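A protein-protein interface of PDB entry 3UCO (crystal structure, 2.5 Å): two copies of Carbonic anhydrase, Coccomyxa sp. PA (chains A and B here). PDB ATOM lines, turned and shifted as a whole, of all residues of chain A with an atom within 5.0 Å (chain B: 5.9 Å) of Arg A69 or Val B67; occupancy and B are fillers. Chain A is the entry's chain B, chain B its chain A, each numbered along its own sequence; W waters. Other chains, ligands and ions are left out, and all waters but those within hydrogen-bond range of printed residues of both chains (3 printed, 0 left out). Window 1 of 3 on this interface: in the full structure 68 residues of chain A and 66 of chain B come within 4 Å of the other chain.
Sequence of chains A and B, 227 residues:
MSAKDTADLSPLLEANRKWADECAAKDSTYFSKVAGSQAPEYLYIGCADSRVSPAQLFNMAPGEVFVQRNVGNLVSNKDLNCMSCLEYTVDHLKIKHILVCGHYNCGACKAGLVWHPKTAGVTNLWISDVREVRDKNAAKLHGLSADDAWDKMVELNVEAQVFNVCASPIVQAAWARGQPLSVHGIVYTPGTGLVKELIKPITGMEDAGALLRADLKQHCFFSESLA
Val A67 touches Arg B69, and with the chains exchanged Arg A69 touches Val B67.
Gln A68 touches Arg B69, and with the chains exchanged Arg A69 touches Gln B68.
Arg B69 touches its own counterpart, Arg A69.
Positions printed for both chains: 44, 54, 67, 68 and 69.
Of the 15 pairs that touch across the chains among the printed residues, 5 have their exchanged pair printed and touching as well.
Phe B66 touches Ala A48 (CE2 to CB, 3.4 Å).
Ala A48 touches Cys B85.
CA of Asp A49 touches CE1 of Phe B66, at 3.9 Å.
Ser A50 touches Val B65.
Ser A50 touches Phe B66.
Ser A53 touches Ala B55.
Val A67 touches Arg B69 (O to CB, 3.4 Å).
Arg A69 touches Val B67.
N of Arg A69 touches O of Arg B69 (3.8 Å).
OD1 of Asn B81 touches CB of Asn A70, 3.3 Å away.
The backbone NH of Phe B66 sits at hydrogen-bond distance from the backbone carbonyl oxygen of Tyr B42 (2.8 Å).
The backbone NH (N) of Gln B68 is in hydrogen-bond range of the backbone carbonyl oxygen (O) of Tyr B44, at 2.9 Å.
O of Asn B81 is in hydrogen-bond range of SG of Cys B85 (3.7 Å).
N of Gly A46 lies within hydrogen-bond range of O of Gln A68 (3.0 Å).
The side-chain sulfur (SG) of Cys A47 lies close to the backbone NH (N) of Asp A49, 3.5 Å away.
The backbone NH (N) of Ala A48 lies within hydrogen-bond range of the backbone carbonyl oxygen (O) of Asn A70, 2.8 Å away.
Of the 13 printed residues of chain B, 8 touch a printed residue of chain A.
Of the 14 printed residues of chain A, 9 touch a printed residue of chain B.
Among the printed residues, 15 pairs touch across the chains.
Among the printed residues, no Asp or Glu carboxylate lies within 4 Å of a Lys or Arg side-chain nitrogen of the other chain.
Gly A46 touches none of the printed residues of chain B.
Val A52 touches none of the printed residues of chain B.
Printed residues of chain B within 4 Å of Val A67: Arg B69.
Of the printed residues of chain B, Arg A69 touches Val B67, Gln B68 and Arg B69.
Of the printed residues of chain A, Phe B66 touches Ala A48 (3.4 Å), Asp A49 (3.9 Å) and Ser A50 (3.7 Å).
Of chain A, only Ala A48 (3.1 Å) and Arg A69 (3.4 Å) come within 4 Å of Val B67.
Of the printed residues of chain A, Gln B68 touches Arg A69.
Of the printed residues of chain A, Arg B69 touches Val A67, Gln A68 and Arg A69.
Of the printed residues of chain A, Cys B85 touches Ala A48 and Val A71.
The nearest residue of chain B that does not touch Arg A69 is Val B65 (4.3 Å).
The nearest printed residue of chain A that does not touch Phe B66 is Val A71 (4.2 Å).
Water W3 lies within hydrogen-bond range of the backbone carbonyl oxygen (O) of Asn B81, the backbone NH (N) of Val A71 and the side-chain sulfur (SG) of Cys B85.
Water W1 bridges O of Ser A50 and N of Val B65.
Water W2 lies within hydrogen-bond range of the backbone carbonyl oxygen of Val B65 (2.8 Å), the side-chain hydroxyl of Ser A53 (2.9 Å) and the guanidinium group of Arg A69 (2.9 Å).
The backbone NH (N) of Val B67 sits at hydrogen-bond distance from the backbone carbonyl oxygen (O) of Ala A48, 3.1 Å away.
The side-chain amide nitrogen (NE2) of Gln B68 lies within hydrogen-bond range of the backbone carbonyl oxygen (O) of Arg A69.
The side-chain amide nitrogen (NE2) of Gln A68 lies within hydrogen-bond range of the backbone carbonyl oxygen (O) of Arg B69 (3.0 Å).
OE1 of Gln A68 is in hydrogen-bond range of ND2 of Asn B81, 3.1 Å away.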
ATOM      1  N   TYR A  44      -5.895  21.072  24.611  1.00  0.00           N
ATOM      2  CA  TYR A  44      -5.014  21.123  23.469  1.00  0.00           C
ATOM      3  C   TYR A  44      -5.763  20.526  22.260  1.00  0.00           C
ATOM      4  O   TYR A  44      -6.371  19.428  22.340  1.00  0.00           O
ATOM      5  CB  TYR A  44      -3.780  20.275  23.808  1.00  0.00           C
ATOM      6  CG  TYR A  44      -2.833  20.018  22.656  1.00  0.00           C
ATOM      7  CD1 TYR A  44      -1.743  20.835  22.438  1.00  0.00           C
ATOM      8  CD2 TYR A  44      -3.047  18.950  21.775  1.00  0.00           C
ATOM      9  CE1 TYR A  44      -0.865  20.621  21.382  1.00  0.00           C
ATOM     10  CE2 TYR A  44      -2.152  18.693  20.720  1.00  0.00           C
ATOM     11  CZ  TYR A  44      -1.048  19.518  20.549  1.00  0.00           C
ATOM     12  OH  TYR A  44      -0.202  19.293  19.490  1.00  0.00           O
ATOM     13  N   GLY A  46      -4.782  19.171  18.581  1.00  0.00           N
ATOM     14  CA  GLY A  46      -3.638  19.039  17.688  1.00  0.00           C
ATOM     15  C   GLY A  46      -3.750  17.875  16.717  1.00  0.00           C
ATOM     16  O   GLY A  46      -4.782  17.172  16.693  1.00  0.00           O
ATOM     17  N   CYS A  47      -2.697  17.624  15.944  1.00  0.00           N
ATOM     18  CA  CYS A  47      -2.771  16.568  14.943  1.00  0.00           C
ATOM     19  C   CYS A  47      -2.495  15.181  15.578  1.00  0.00           C
ATOM     20  O   CYS A  47      -1.721  15.035  16.556  1.00  0.00           O
ATOM     21  CB  CYS A  47      -1.831  16.881  13.788  1.00  0.00           C
ATOM     22  SG  CYS A  47      -1.905  15.644  12.440  1.00  0.00           S
ATOM     23  N   ALA A  48      -3.154  14.174  15.033  1.00  0.00           N
ATOM     24  CA  ALA A  48      -2.940  12.796  15.434  1.00  0.00           C
ATOM     25  C   ALA A  48      -1.490  12.261  15.142  1.00  0.00           C
ATOM     26  O   ALA A  48      -1.132  11.196  15.611  1.00  0.00           O
ATOM     27  CB  ALA A  48      -3.939  11.922  14.710  1.00  0.00           C
ATOM     28  N   ASP A  49      -0.732  12.985  14.311  1.00  0.00           N
ATOM     29  CA  ASP A  49       0.630  12.655  13.904  1.00  0.00           C
ATOM     30  C   ASP A  49       1.497  12.197  15.059  1.00  0.00           C
ATOM     31  O   ASP A  49       1.640  12.916  16.033  1.00  0.00           O
ATOM     32  CB  ASP A  49       1.244  13.904  13.304  1.00  0.00           C
ATOM     33  CG  ASP A  49       2.603  13.667  12.670  1.00  0.00           C
ATOM     34  OD1 ASP A  49       3.629  13.555  13.405  1.00  0.00           O
ATOM     35  OD2 ASP A  49       2.627  13.709  11.417  1.00  0.00           O
ATOM     36  N   SER A  50       2.094  11.005  14.914  1.00  0.00           N
ATOM     37  CA  SER A  50       2.898  10.324  15.967  1.00  0.00           C
ATOM     38  C   SER A  50       4.127  11.069  16.454  1.00  0.00           C
ATOM     39  O   SER A  50       4.729  10.675  17.428  1.00  0.00           O
ATOM     40  CB  SER A  50       3.405   9.011  15.390  1.00  0.00           C
ATOM     41  OG  SER A  50       4.224   9.270  14.252  1.00  0.00           O
ATOM     42  N   VAL A  52       4.006  14.232  17.545  1.00  0.00           N
ATOM     43  CA  VAL A  52       3.552  15.469  18.239  1.00  0.00           C
ATOM     44  C   VAL A  52       2.720  15.140  19.461  1.00  0.00           C
ATOM     45  O   VAL A  52       1.492  14.966  19.380  1.00  0.00           O
ATOM     46  CB  VAL A  52       2.794  16.414  17.274  1.00  0.00           C
ATOM     47  CG1 VAL A  52       2.557  17.761  17.924  1.00  0.00           C
ATOM     48  CG2 VAL A  52       3.549  16.588  15.898  1.00  0.00           C
ATOM     49  N   SER A  53       3.374  15.036  20.602  1.00  0.00           N
ATOM     50  CA  SER A  53       2.705  14.576  21.810  1.00  0.00           C
ATOM     51  C   SER A  53       2.603  15.675  22.840  1.00  0.00           C
ATOM     52  O   SER A  53       3.537  15.928  23.557  1.00  0.00           O
ATOM     53  CB  SER A  53       3.433  13.370  22.402  1.00  0.00           C
ATOM     54  OG  SER A  53       3.657  12.405  21.360  1.00  0.00           O
ATOM     55  N   PRO A  54       1.439  16.302  22.974  1.00  0.00           N
ATOM     56  CA  PRO A  54       1.475  17.495  23.820  1.00  0.00           C
ATOM     57  C   PRO A  54       2.027  17.303  25.238  1.00  0.00           C
ATOM     58  O   PRO A  54       2.789  18.170  25.702  1.00  0.00           O
ATOM     59  CB  PRO A  54       0.017  17.962  23.854  1.00  0.00           C
ATOM     60  CG  PRO A  54      -0.802  16.812  23.393  1.00  0.00           C
ATOM     61  CD  PRO A  54       0.072  15.883  22.610  1.00  0.00           C
ATOM     62  N   VAL A  67      -6.966  16.588  26.038  1.00  0.00           N
ATOM     63  CA  VAL A  67      -6.507  16.509  24.645  1.00  0.00           C
ATOM     64  C   VAL A  67      -7.497  16.009  23.566  1.00  0.00           C
ATOM     65  O   VAL A  67      -7.980  14.845  23.608  1.00  0.00           O
ATOM     66  CB  VAL A  67      -5.186  15.679  24.619  1.00  0.00           C
ATOM     67  CG1 VAL A  67      -4.719  15.371  23.219  1.00  0.00           C
ATOM     68  CG2 VAL A  67      -4.107  16.417  25.410  1.00  0.00           C
ATOM     69  N   GLN A  68      -7.697  16.830  22.537  1.00  0.00           N
ATOM     70  CA  GLN A  68      -8.258  16.316  21.264  1.00  0.00           C
ATOM     71  C   GLN A  68      -7.133  16.160  20.173  1.00  0.00           C
ATOM     72  O   GLN A  68      -6.317  17.045  19.971  1.00  0.00           O
ATOM     73  CB  GLN A  68      -9.387  17.204  20.807  1.00  0.00           C
ATOM     74  CG  GLN A  68      -9.685  17.252  19.306  1.00  0.00           C
ATOM     75  CD  GLN A  68     -10.525  16.090  18.709  1.00  0.00           C
ATOM     76  OE1 GLN A  68     -10.768  16.099  17.513  1.00  0.00           O
ATOM     77  NE2 GLN A  68     -10.931  15.087  19.522  1.00  0.00           N
ATOM     78  N   ARG A  69      -7.072  15.032  19.474  1.00  0.00           N
ATOM     79  CA  ARG A  69      -6.082  14.884  18.421  1.00  0.00           C
ATOM     80  C   ARG A  69      -6.811  14.263  17.242  1.00  0.00           C
ATOM     81  O   ARG A  69      -7.493  13.275  17.395  1.00  0.00           O
ATOM     82  CB  ARG A  69      -4.872  14.011  18.862  1.00  0.00           C
ATOM     83  CG  ARG A  69      -3.731  14.881  19.413  1.00  0.00           C
ATOM     84  CD  ARG A  69      -2.602  14.108  20.072  1.00  0.00           C
ATOM     85  NE  ARG A  69      -1.589  13.675  19.093  1.00  0.00           N
ATOM     86  CZ  ARG A  69      -0.580  12.835  19.376  1.00  0.00           C
ATOM     87  NH1 ARG A  69      -0.402  12.381  20.628  1.00  0.00           N
ATOM     88  NH2 ARG A  69       0.277  12.478  18.409  1.00  0.00           N
ATOM     89  N   ASN A  70      -6.659  14.847  16.073  1.00  0.00           N
ATOM     90  CA  ASN A  70      -7.303  14.323  14.928  1.00  0.00           C
ATOM     91  C   ASN A  70      -6.420  14.628  13.728  1.00  0.00           C
ATOM     92  O   ASN A  70      -5.455  15.337  13.856  1.00  0.00           O
ATOM     93  CB  ASN A  70      -8.741  14.910  14.815  1.00  0.00           C
ATOM     94  CG  ASN A  70      -8.739  16.389  14.457  1.00  0.00           C
ATOM     95  OD1 ASN A  70      -8.086  16.814  13.483  1.00  0.00           O
ATOM     96  ND2 ASN A  70      -9.441  17.196  15.260  1.00  0.00           N
ATOM     97  N   VAL A  71      -6.751  14.101  12.554  1.00  0.00           N
ATOM     98  CA  VAL A  71      -5.887  14.272  11.366  1.00  0.00           C
ATOM     99  C   VAL A  71      -6.061  15.688  10.814  1.00  0.00           C
ATOM    100  O   VAL A  71      -7.160  16.047  10.273  1.00  0.00           O
ATOM    101  CB  VAL A  71      -6.345  13.238  10.281  1.00  0.00           C
ATOM    102  CG1 VAL A  71      -5.851  13.641   8.869  1.00  0.00           C
ATOM    103  CG2 VAL A  71      -5.987  11.837  10.716  1.00  0.00           C
ATOM    104  N   TYR B  42       2.139   1.705  16.099  1.00  0.00           N
ATOM    105  CA  TYR B  42       0.896   1.742  16.878  1.00  0.00           C
ATOM    106  C   TYR B  42      -0.030   2.876  16.464  1.00  0.00           C
ATOM    107  O   TYR B  42       0.430   4.048  16.260  1.00  0.00           O
ATOM    108  CB  TYR B  42       1.168   1.896  18.394  1.00  0.00           C
ATOM    109  CG  TYR B  42       1.979   0.751  18.904  1.00  0.00           C
ATOM    110  CD1 TYR B  42       1.375  -0.460  19.244  1.00  0.00           C
ATOM    111  CD2 TYR B  42       3.354   0.840  18.944  1.00  0.00           C
ATOM    112  CE1 TYR B  42       2.132  -1.555  19.659  1.00  0.00           C
ATOM    113  CE2 TYR B  42       4.104  -0.221  19.308  1.00  0.00           C
ATOM    114  CZ  TYR B  42       3.499  -1.415  19.676  1.00  0.00           C
ATOM    115  OH  TYR B  42       4.300  -2.433  20.081  1.00  0.00           O
ATOM    116  N   LEU B  43      -1.314   2.531  16.367  1.00  0.00           N
ATOM    117  CA  LEU B  43      -2.359   3.504  16.433  1.00  0.00           C
ATOM    118  C   LEU B  43      -2.917   3.397  17.836  1.00  0.00           C
ATOM    119  O   LEU B  43      -3.239   2.315  18.298  1.00  0.00           O
ATOM    120  CB  LEU B  43      -3.472   3.203  15.425  1.00  0.00           C
ATOM    121  CG  LEU B  43      -4.798   3.962  15.671  1.00  0.00           C
ATOM    122  CD1 LEU B  43      -4.558   5.453  15.921  1.00  0.00           C
ATOM    123  CD2 LEU B  43      -5.854   3.755  14.553  1.00  0.00           C
ATOM    124  N   TYR B  44      -3.118   4.505  18.527  1.00  0.00           N
ATOM    125  CA  TYR B  44      -3.728   4.365  19.829  1.00  0.00           C
ATOM    126  C   TYR B  44      -5.020   5.148  19.888  1.00  0.00           C
ATOM    127  O   TYR B  44      -5.031   6.297  19.505  1.00  0.00           O
ATOM    128  CB  TYR B  44      -2.749   4.823  20.846  1.00  0.00           C
ATOM    129  CG  TYR B  44      -3.299   5.175  22.185  1.00  0.00           C
ATOM    130  CD1 TYR B  44      -2.989   4.365  23.321  1.00  0.00           C
ATOM    131  CD2 TYR B  44      -4.070   6.328  22.357  1.00  0.00           C
ATOM    132  CE1 TYR B  44      -3.436   4.703  24.573  1.00  0.00           C
ATOM    133  CE2 TYR B  44      -4.532   6.696  23.619  1.00  0.00           C
ATOM    134  CZ  TYR B  44      -4.200   5.877  24.739  1.00  0.00           C
ATOM    135  OH  TYR B  44      -4.666   6.198  26.003  1.00  0.00           O
ATOM    136  N   ILE B  45      -6.108   4.507  20.328  1.00  0.00           N
ATOM    137  CA  ILE B  45      -7.393   5.152  20.508  1.00  0.00           C
ATOM    138  C   ILE B  45      -7.729   5.192  22.031  1.00  0.00           C
ATOM    139  O   ILE B  45      -7.979   4.153  22.638  1.00  0.00           O
ATOM    140  CB  ILE B  45      -8.508   4.393  19.740  1.00  0.00           C
ATOM    141  CG1 ILE B  45      -8.224   4.400  18.244  1.00  0.00           C
ATOM    142  CG2 ILE B  45      -9.907   5.009  20.051  1.00  0.00           C
ATOM    143  CD1 ILE B  45      -8.983   3.298  17.444  1.00  0.00           C
ATOM    144  N   PRO B  54      -0.754   8.572  26.164  1.00  0.00           N
ATOM    145  CA  PRO B  54      -0.137   7.339  25.794  1.00  0.00           C
ATOM    146  C   PRO B  54       1.373   7.527  25.635  1.00  0.00           C
ATOM    147  O   PRO B  54       2.125   6.623  26.010  1.00  0.00           O
ATOM    148  CB  PRO B  54      -0.779   7.004  24.453  1.00  0.00           C
ATOM    149  CG  PRO B  54      -1.449   8.304  24.002  1.00  0.00           C
ATOM    150  CD  PRO B  54      -1.812   8.998  25.241  1.00  0.00           C
ATOM    151  N   ALA B  55       1.815   8.638  25.097  1.00  0.00           N
ATOM    152  CA  ALA B  55       3.221   8.783  24.816  1.00  0.00           C
ATOM    153  C   ALA B  55       4.046   8.682  26.060  1.00  0.00           C
ATOM    154  O   ALA B  55       5.127   8.166  26.042  1.00  0.00           O
ATOM    155  CB  ALA B  55       3.486  10.072  24.135  1.00  0.00           C
ATOM    156  N   VAL B  65       3.822   6.346  18.171  1.00  0.00           N
ATOM    157  CA  VAL B  65       2.404   6.077  18.320  1.00  0.00           C
ATOM    158  C   VAL B  65       1.544   7.213  17.706  1.00  0.00           C
ATOM    159  O   VAL B  65       1.650   8.401  18.061  1.00  0.00           O
ATOM    160  CB  VAL B  65       2.087   5.824  19.778  1.00  0.00           C
ATOM    161  CG1 VAL B  65       2.316   7.102  20.594  1.00  0.00           C
ATOM    162  CG2 VAL B  65       0.655   5.353  19.939  1.00  0.00           C
ATOM    163  N   PHE B  66       0.705   6.830  16.758  1.00  0.00           N
ATOM    164  CA  PHE B  66      -0.236   7.741  16.141  1.00  0.00           C
ATOM    165  C   PHE B  66      -1.489   7.721  17.053  1.00  0.00           C
ATOM    166  O   PHE B  66      -1.993   6.597  17.395  1.00  0.00           O
ATOM    167  CB  PHE B  66      -0.568   7.175  14.793  1.00  0.00           C
ATOM    168  CG  PHE B  66      -1.218   8.140  13.849  1.00  0.00           C
ATOM    169  CD1 PHE B  66      -0.444   8.875  12.923  1.00  0.00           C
ATOM    170  CD2 PHE B  66      -2.613   8.293  13.829  1.00  0.00           C
ATOM    171  CE1 PHE B  66      -1.050   9.762  11.992  1.00  0.00           C
ATOM    172  CE2 PHE B  66      -3.233   9.178  12.901  1.00  0.00           C
ATOM    173  CZ  PHE B  66      -2.471   9.908  11.984  1.00  0.00           C
ATOM    174  N   VAL B  67      -1.992   8.897  17.457  1.00  0.00           N
ATOM    175  CA  VAL B  67      -2.994   8.969  18.506  1.00  0.00           C
ATOM    176  C   VAL B  67      -4.366   9.618  18.092  1.00  0.00           C
ATOM    177  O   VAL B  67      -4.412  10.787  17.616  1.00  0.00           O
ATOM    178  CB  VAL B  67      -2.405   9.751  19.677  1.00  0.00           C
ATOM    179  CG1 VAL B  67      -3.477  10.134  20.692  1.00  0.00           C
ATOM    180  CG2 VAL B  67      -1.333   8.900  20.378  1.00  0.00           C
ATOM    181  N   GLN B  68      -5.463   8.863  18.295  1.00  0.00           N
ATOM    182  CA  GLN B  68      -6.796   9.444  18.421  1.00  0.00           C
ATOM    183  C   GLN B  68      -7.225   9.555  19.911  1.00  0.00           C
ATOM    184  O   GLN B  68      -7.121   8.603  20.676  1.00  0.00           O
ATOM    185  CB  GLN B  68      -7.810   8.705  17.546  1.00  0.00           C
ATOM    186  CG  GLN B  68      -9.260   8.765  18.003  1.00  0.00           C
ATOM    187  CD  GLN B  68     -10.123   9.996  17.512  1.00  0.00           C
ATOM    188  OE1 GLN B  68     -11.274  10.136  17.914  1.00  0.00           O
ATOM    189  NE2 GLN B  68      -9.563  10.847  16.717  1.00  0.00           N
ATOM    190  N   ARG B  69      -7.678  10.732  20.324  1.00  0.00           N
ATOM    191  CA  ARG B  69      -8.238  10.892  21.656  1.00  0.00           C
ATOM    192  C   ARG B  69      -9.594  11.642  21.585  1.00  0.00           C
ATOM    193  O   ARG B  69      -9.703  12.728  20.993  1.00  0.00           O
ATOM    194  CB  ARG B  69      -7.272  11.653  22.543  1.00  0.00           C
ATOM    195  CG  ARG B  69      -6.257  10.743  23.160  1.00  0.00           C
ATOM    196  CD  ARG B  69      -5.082  11.429  23.848  1.00  0.00           C
ATOM    197  NE  ARG B  69      -5.486  11.827  25.184  1.00  0.00           N
ATOM    198  CZ  ARG B  69      -4.675  12.494  26.019  1.00  0.00           C
ATOM    199  NH1 ARG B  69      -3.400  12.768  25.650  1.00  0.00           N
ATOM    200  NH2 ARG B  69      -5.097  12.793  27.245  1.00  0.00           N
ATOM    201  N   ASN B  81     -14.035  11.370  12.185  1.00  0.00           N
ATOM    202  CA  ASN B  81     -12.879  11.926  12.822  1.00  0.00           C
ATOM    203  C   ASN B  81     -12.022  10.700  13.263  1.00  0.00           C
ATOM    204  O   ASN B  81     -10.815  10.638  12.957  1.00  0.00           O
ATOM    205  CB  ASN B  81     -13.338  12.836  13.954  1.00  0.00           C
ATOM    206  CG  ASN B  81     -12.220  13.335  14.851  1.00  0.00           C
ATOM    207  OD1 ASN B  81     -11.195  12.699  15.020  1.00  0.00           O
ATOM    208  ND2 ASN B  81     -12.454  14.484  15.501  1.00  0.00           N
ATOM    209  N   CYS B  85      -8.556   8.485  11.230  1.00  0.00           N
ATOM    210  CA  CYS B  85      -7.353   8.140  11.926  1.00  0.00           C
ATOM    211  C   CYS B  85      -7.083   6.688  11.656  1.00  0.00           C
ATOM    212  O   CYS B  85      -5.981   6.276  11.492  1.00  0.00           O
ATOM    213  CB  CYS B  85      -7.525   8.352  13.410  1.00  0.00           C
ATOM    214  SG  CYS B  85      -7.272  10.040  13.978  1.00  0.00           S
HETATM  215  O   HOH W   1       4.892   8.834  19.501  1.00  0.00           O
HETATM  216  O   HOH W   2       2.020  10.597  19.807  1.00  0.00           O
HETATM  217  O   HOH W   3      -9.163  12.403  12.314  1.00  0.00           O
